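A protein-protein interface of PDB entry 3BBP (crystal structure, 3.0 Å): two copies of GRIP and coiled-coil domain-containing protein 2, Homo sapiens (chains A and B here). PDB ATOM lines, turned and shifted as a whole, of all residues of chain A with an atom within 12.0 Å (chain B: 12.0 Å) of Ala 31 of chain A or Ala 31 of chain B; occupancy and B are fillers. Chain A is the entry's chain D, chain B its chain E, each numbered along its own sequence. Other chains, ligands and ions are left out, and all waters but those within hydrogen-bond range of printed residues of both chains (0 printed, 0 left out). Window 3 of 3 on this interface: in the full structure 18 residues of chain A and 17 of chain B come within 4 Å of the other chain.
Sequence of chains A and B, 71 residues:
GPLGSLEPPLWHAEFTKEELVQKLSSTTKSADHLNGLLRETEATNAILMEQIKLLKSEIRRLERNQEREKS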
ATOM      1  N   LYS A  29      -5.837   1.175 -33.558  1.00  0.00           N
ATOM      2  CA  LYS A  29      -4.969   0.080 -33.975  1.00  0.00           C
ATOM      3  C   LYS A  29      -3.556   0.229 -33.417  1.00  0.00           C
ATOM      4  O   LYS A  29      -2.817  -0.750 -33.303  1.00  0.00           O
ATOM      5  CB  LYS A  29      -4.926  -0.025 -35.503  1.00  0.00           C
ATOM      6  CG  LYS A  29      -6.136  -0.721 -36.112  1.00  0.00           C
ATOM      7  CD  LYS A  29      -5.800  -1.318 -37.470  1.00  0.00           C
ATOM      8  CE  LYS A  29      -6.798  -2.402 -37.858  1.00  0.00           C
ATOM      9  NZ  LYS A  29      -6.370  -3.157 -39.071  1.00  0.00           N
ATOM     10  N   SER A  30      -3.186   1.456 -33.070  1.00  0.00           N
ATOM     11  CA  SER A  30      -1.858   1.722 -32.523  1.00  0.00           C
ATOM     12  C   SER A  30      -1.825   1.520 -31.009  1.00  0.00           C
ATOM     13  O   SER A  30      -0.769   1.620 -30.382  1.00  0.00           O
ATOM     14  CB  SER A  30      -1.395   3.134 -32.886  1.00  0.00           C
ATOM     15  OG  SER A  30      -2.282   4.110 -32.370  1.00  0.00           O
ATOM     16  N   ALA A  31      -2.987   1.234 -30.430  1.00  0.00           N
ATOM     17  CA  ALA A  31      -3.074   0.906 -29.012  1.00  0.00           C
ATOM     18  C   ALA A  31      -2.435  -0.454 -28.762  1.00  0.00           C
ATOM     19  O   ALA A  31      -2.559  -1.024 -27.676  1.00  0.00           O
ATOM     20  CB  ALA A  31      -4.523   0.903 -28.555  1.00  0.00           C
ATOM     21  N   ASP A  32      -1.753  -0.967 -29.781  1.00  0.00           N
ATOM     22  CA  ASP A  32      -1.106  -2.270 -29.708  1.00  0.00           C
ATOM     23  C   ASP A  32       0.370  -2.126 -29.348  1.00  0.00           C
ATOM     24  O   ASP A  32       0.863  -2.796 -28.440  1.00  0.00           O
ATOM     25  CB  ASP A  32      -1.254  -3.015 -31.037  1.00  0.00           C
ATOM     26  CG  ASP A  32      -2.706  -3.205 -31.446  1.00  0.00           C
ATOM     27  OD1 ASP A  32      -3.580  -2.493 -30.908  1.00  0.00           O
ATOM     28  OD2 ASP A  32      -2.973  -4.066 -32.310  1.00  0.00           O
ATOM     29  N   HIS A  33       1.070  -1.246 -30.060  1.00  0.00           N
ATOM     30  CA  HIS A  33       2.490  -1.011 -29.811  1.00  0.00           C
ATOM     31  C   HIS A  33       2.726  -0.424 -28.429  1.00  0.00           C
ATOM     32  O   HIS A  33       3.864  -0.324 -27.975  1.00  0.00           O
ATOM     33  CB  HIS A  33       3.082  -0.086 -30.875  1.00  0.00           C
ATOM     34  CG  HIS A  33       3.153  -0.704 -32.234  1.00  0.00           C
ATOM     35  ND1 HIS A  33       2.084  -0.714 -33.105  1.00  0.00           N
ATOM     36  CD2 HIS A  33       4.164  -1.340 -32.874  1.00  0.00           C
ATOM     37  CE1 HIS A  33       2.434  -1.326 -34.221  1.00  0.00           C
ATOM     38  NE2 HIS A  33       3.690  -1.715 -34.107  1.00  0.00           N
ATOM     39  N   LEU A  34       1.644  -0.033 -27.764  1.00  0.00           N
ATOM     40  CA  LEU A  34       1.738   0.524 -26.421  1.00  0.00           C
ATOM     41  C   LEU A  34       1.971  -0.567 -25.378  1.00  0.00           C
ATOM     42  O   LEU A  34       2.521  -0.303 -24.311  1.00  0.00           O
ATOM     43  CB  LEU A  34       0.486   1.337 -26.082  1.00  0.00           C
ATOM     44  CG  LEU A  34       0.239   2.565 -26.964  1.00  0.00           C
ATOM     45  CD1 LEU A  34      -0.990   3.331 -26.501  1.00  0.00           C
ATOM     46  CD2 LEU A  34       1.461   3.472 -26.977  1.00  0.00           C
ATOM     47  N   ASN A  35       1.559  -1.790 -25.693  1.00  0.00           N
ATOM     48  CA  ASN A  35       1.748  -2.916 -24.780  1.00  0.00           C
ATOM     49  C   ASN A  35       3.123  -3.565 -24.892  1.00  0.00           C
ATOM     50  O   ASN A  35       3.834  -3.710 -23.898  1.00  0.00           O
ATOM     51  CB  ASN A  35       0.659  -3.970 -24.981  1.00  0.00           C
ATOM     52  CG  ASN A  35      -0.647  -3.584 -24.324  1.00  0.00           C
ATOM     53  OD1 ASN A  35      -1.148  -2.475 -24.515  1.00  0.00           O
ATOM     54  ND2 ASN A  35      -1.208  -4.502 -23.541  1.00  0.00           N
ATOM     55  N   GLY A  36       3.490  -3.959 -26.106  1.00  0.00           N
ATOM     56  CA  GLY A  36       4.786  -4.563 -26.344  1.00  0.00           C
ATOM     57  C   GLY A  36       5.918  -3.681 -25.851  1.00  0.00           C
ATOM     58  O   GLY A  36       6.965  -4.179 -25.435  1.00  0.00           O
ATOM     59  N   LEU A  37       5.703  -2.369 -25.892  1.00  0.00           N
ATOM     60  CA  LEU A  37       6.721  -1.411 -25.467  1.00  0.00           C
ATOM     61  C   LEU A  37       6.692  -1.171 -23.963  1.00  0.00           C
ATOM     62  O   LEU A  37       7.736  -1.023 -23.330  1.00  0.00           O
ATOM     63  CB  LEU A  37       6.573  -0.087 -26.219  1.00  0.00           C
ATOM     64  CG  LEU A  37       6.913  -0.127 -27.710  1.00  0.00           C
ATOM     65  CD1 LEU A  37       7.064   1.284 -28.257  1.00  0.00           C
ATOM     66  CD2 LEU A  37       8.181  -0.935 -27.952  1.00  0.00           C
ATOM     67  N   LEU A  38       5.492  -1.128 -23.392  1.00  0.00           N
ATOM     68  CA  LEU A  38       5.344  -0.975 -21.952  1.00  0.00           C
ATOM     69  C   LEU A  38       6.001  -2.137 -21.219  1.00  0.00           C
ATOM     70  O   LEU A  38       6.663  -1.947 -20.199  1.00  0.00           O
ATOM     71  CB  LEU A  38       3.868  -0.904 -21.569  1.00  0.00           C
ATOM     72  CG  LEU A  38       3.595  -0.784 -20.071  1.00  0.00           C
ATOM     73  CD1 LEU A  38       3.660   0.673 -19.621  1.00  0.00           C
ATOM     74  CD2 LEU A  38       2.248  -1.397 -19.728  1.00  0.00           C
ATOM     75  N   ARG A  39       5.809  -3.344 -21.745  1.00  0.00           N
ATOM     76  CA  ARG A  39       6.386  -4.541 -21.150  1.00  0.00           C
ATOM     77  C   ARG A  39       7.909  -4.536 -21.253  1.00  0.00           C
ATOM     78  O   ARG A  39       8.590  -5.181 -20.458  1.00  0.00           O
ATOM     79  CB  ARG A  39       5.812  -5.797 -21.806  1.00  0.00           C
ATOM     80  CG  ARG A  39       4.297  -5.891 -21.730  1.00  0.00           C
ATOM     81  CD  ARG A  39       3.789  -7.201 -22.308  1.00  0.00           C
ATOM     82  NE  ARG A  39       2.331  -7.226 -22.401  1.00  0.00           N
ATOM     83  CZ  ARG A  39       1.625  -8.273 -22.819  1.00  0.00           C
ATOM     84  NH1 ARG A  39       2.241  -9.388 -23.183  1.00  0.00           N
ATOM     85  NH2 ARG A  39       0.302  -8.204 -22.873  1.00  0.00           N
ATOM     86  N   SER B  30      -9.327   3.479 -24.575  1.00  0.00           N
ATOM     87  CA  SER B  30      -8.462   3.062 -23.476  1.00  0.00           C
ATOM     88  C   SER B  30      -6.989   3.139 -23.868  1.00  0.00           C
ATOM     89  O   SER B  30      -6.105   2.899 -23.045  1.00  0.00           O
ATOM     90  CB  SER B  30      -8.818   1.648 -23.011  1.00  0.00           C
ATOM     91  OG  SER B  30      -8.669   0.712 -24.063  1.00  0.00           O
ATOM     92  N   ALA B  31      -6.732   3.476 -25.128  1.00  0.00           N
ATOM     93  CA  ALA B  31      -5.368   3.691 -25.598  1.00  0.00           C
ATOM     94  C   ALA B  31      -4.808   4.964 -24.975  1.00  0.00           C
ATOM     95  O   ALA B  31      -3.746   5.452 -25.368  1.00  0.00           O
ATOM     96  CB  ALA B  31      -5.338   3.783 -27.112  1.00  0.00           C
ATOM     97  N   ASP B  32      -5.536   5.497 -23.999  1.00  0.00           N
ATOM     98  CA  ASP B  32      -5.149   6.727 -23.322  1.00  0.00           C
ATOM     99  C   ASP B  32      -4.404   6.426 -22.024  1.00  0.00           C
ATOM    100  O   ASP B  32      -3.333   6.978 -21.772  1.00  0.00           O
ATOM    101  CB  ASP B  32      -6.380   7.590 -23.034  1.00  0.00           C
ATOM    102  CG  ASP B  32      -7.160   7.939 -24.291  1.00  0.00           C
ATOM    103  OD1 ASP B  32      -6.968   7.263 -25.325  1.00  0.00           O
ATOM    104  OD2 ASP B  32      -7.969   8.890 -24.244  1.00  0.00           O
ATOM    105  N   HIS B  33      -4.975   5.548 -21.204  1.00  0.00           N
ATOM    106  CA  HIS B  33      -4.362   5.171 -19.933  1.00  0.00           C
ATOM    107  C   HIS B  33      -3.035   4.455 -20.140  1.00  0.00           C
ATOM    108  O   HIS B  33      -2.290   4.224 -19.189  1.00  0.00           O
ATOM    109  CB  HIS B  33      -5.308   4.287 -19.118  1.00  0.00           C
ATOM    110  CG  HIS B  33      -6.522   5.006 -18.620  1.00  0.00           C
ATOM    111  ND1 HIS B  33      -7.651   5.179 -19.391  1.00  0.00           N
ATOM    112  CD2 HIS B  33      -6.782   5.599 -17.432  1.00  0.00           C
ATOM    113  CE1 HIS B  33      -8.556   5.847 -18.698  1.00  0.00           C
ATOM    114  NE2 HIS B  33      -8.052   6.114 -17.504  1.00  0.00           N
ATOM    115  N   LEU B  34      -2.744   4.105 -21.387  1.00  0.00           N
ATOM    116  CA  LEU B  34      -1.495   3.436 -21.718  1.00  0.00           C
ATOM    117  C   LEU B  34      -0.323   4.414 -21.728  1.00  0.00           C
ATOM    118  O   LEU B  34       0.822   4.017 -21.523  1.00  0.00           O
ATOM    119  CB  LEU B  34      -1.609   2.719 -23.064  1.00  0.00           C
ATOM    120  CG  LEU B  34      -2.644   1.593 -23.119  1.00  0.00           C
ATOM    121  CD1 LEU B  34      -2.626   0.899 -24.476  1.00  0.00           C
ATOM    122  CD2 LEU B  34      -2.410   0.594 -21.993  1.00  0.00           C
ATOM    123  N   ASN B  35      -0.613   5.690 -21.961  1.00  0.00           N
ATOM    124  CA  ASN B  35       0.426   6.718 -21.975  1.00  0.00           C
ATOM    125  C   ASN B  35       0.771   7.252 -20.589  1.00  0.00           C
ATOM    126  O   ASN B  35       1.934   7.256 -20.188  1.00  0.00           O
ATOM    127  CB  ASN B  35       0.038   7.875 -22.895  1.00  0.00           C
ATOM    128  CG  ASN B  35       0.258   7.552 -24.356  1.00  0.00           C
ATOM    129  OD1 ASN B  35      -0.178   6.509 -24.847  1.00  0.00           O
ATOM    130  ND2 ASN B  35       0.940   8.449 -25.061  1.00  0.00           N
ATOM    131  N   GLY B  36      -0.245   7.708 -19.865  1.00  0.00           N
ATOM    132  CA  GLY B  36      -0.049   8.216 -18.521  1.00  0.00           C
ATOM    133  C   GLY B  36       0.648   7.203 -17.635  1.00  0.00           C
ATOM    134  O   GLY B  36       1.393   7.572 -16.727  1.00  0.00           O
ATOM    135  N   LEU B  37       0.411   5.923 -17.907  1.00  0.00           N
ATOM    136  CA  LEU B  37       1.010   4.847 -17.120  1.00  0.00           C
ATOM    137  C   LEU B  37       2.416   4.490 -17.597  1.00  0.00           C
ATOM    138  O   LEU B  37       3.299   4.202 -16.791  1.00  0.00           O
ATOM    139  CB  LEU B  37       0.117   3.605 -17.125  1.00  0.00           C
ATOM    140  CG  LEU B  37      -1.207   3.736 -16.370  1.00  0.00           C
ATOM    141  CD1 LEU B  37      -1.833   2.366 -16.154  1.00  0.00           C
ATOM    142  CD2 LEU B  37      -1.002   4.450 -15.040  1.00  0.00           C
ATOM    143  N   LEU B  38       2.618   4.507 -18.910  1.00  0.00           N
ATOM    144  CA  LEU B  38       3.936   4.245 -19.474  1.00  0.00           C
ATOM    145  C   LEU B  38       4.939   5.281 -18.985  1.00  0.00           C
ATOM    146  O   LEU B  38       6.077   4.950 -18.656  1.00  0.00           O
ATOM    147  CB  LEU B  38       3.881   4.266 -21.000  1.00  0.00           C
ATOM    148  CG  LEU B  38       5.219   4.048 -21.706  1.00  0.00           C
ATOM    149  CD1 LEU B  38       5.513   2.564 -21.857  1.00  0.00           C
ATOM    150  CD2 LEU B  38       5.225   4.738 -23.063  1.00  0.00           C
ATOM    151  N   ARG B  39       4.507   6.538 -18.939  1.00  0.00           N
ATOM    152  CA  ARG B  39       5.361   7.631 -18.490  1.00  0.00           C
ATOM    153  C   ARG B  39       5.698   7.501 -17.007  1.00  0.00           C
ATOM    154  O   ARG B  39       6.715   8.017 -16.549  1.00  0.00           O
ATOM    155  CB  ARG B  39       4.703   8.984 -18.771  1.00  0.00           C
ATOM    156  CG  ARG B  39       4.354   9.201 -20.235  1.00  0.00           C
ATOM    157  CD  ARG B  39       3.793  10.594 -20.476  1.00  0.00           C
ATOM    158  NE  ARG B  39       3.299  10.753 -21.842  1.00  0.00           N
ATOM    159  CZ  ARG B  39       2.809  11.888 -22.334  1.00  0.00           C
ATOM    160  NH1 ARG B  39       2.748  12.974 -21.574  1.00  0.00           N
ATOM    161  NH2 ARG B  39       2.381  11.937 -23.589  1.00  0.00           N
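Lys 29 of chain A touches none of the printed residues of chain B. No residue of chain B comes within 4 Å of Ser 30 of chain A. Ala 31 of chain A touches just these residues of chain B: Ala 31 and Leu 34. Of chain B, only Ala 31 (3.7 Å), Leu 34 (3.5 Å) and Asn 35 (3.7 Å) come within 4 Å of Leu 34 of chain A. Asn 35 of chain A touches one residue of chain B. Leu 37 of chain A touches none of the printed residues of chain B. Of the printed residues of chain B, Leu 38 of chain A touches Leu 38 (3.5 Å). No residue of chain A comes within 4 Å of Ser 30 of chain B. Of the printed residues of chain A, Ala 31 of chain B touches Ala 31 and Leu 34. Asp 32 of chain B touches none of the printed residues of chain A. Printed residues of chain A within 4 Å of Leu 34 of chain B: Ala 31, Leu 34 and Asn 35. Asn 35 of chain B touches just one residue of chain A: Leu 34. Printed residues of chain A within 4 Å of Leu 38 of chain B: Leu 38 (3.5 Å). The nearest residue of chain B that does not touch Ala 31 of chain A is Ser 30 of chain B (5.7 Å). The nearest residue of chain A that does not touch Ala 31 of chain B is Ser 30 of chain A (5.7 Å). The nearest printed residue of chain A that does not touch Leu 38 of chain B is Leu 37 of chain A (4.4 Å).
Ala 31 of chain A touches its own counterpart, Ala 31 of chain B. Ala 31 of chain A touches Leu 34 of chain B, and with the chains exchanged Leu 34 of chain A touches Ala 31 of chain B. Leu 34 of chain B touches its own counterpart, Leu 34 of chain A. Leu 34 of chain A touches Asn 35 of chain B, and with the chains exchanged Asn 35 of chain A touches Leu 34 of chain B.
CB of Ala 31 of chain B touches CB of Ala 31 of chain A (3.3 Å). Leu 34 of chain B touches Ala 31 of chain A (CD1 to O, 3.7 Å). Leu 34 of chain A touches Ala 31 of chain B. Leu 34 of chain B touches Leu 34 of chain A. Leu 34 of chain A touches Asn 35 of chain B. Asn 35 of chain A touches Leu 34 of chain B. CD1 of Leu 38 of chain B touches CD1 of Leu 38 of chain A, 3.5 Å away.
Printed residues of chain B that touch a printed residue of chain A: Ala 31, Leu 34, Asn 35 and Leu 38. Hydrophobic or aromatic side chains of chain B within 4 Å of the printed part of chain A: Ala 31, Leu 34 and Leu 38. Among the printed residues, 7 pairs touch across the chains. Among the printed residues, no Asp or Glu carboxylate lies within 4 Å of a Lys or Arg side-chain nitrogen of the other chain.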
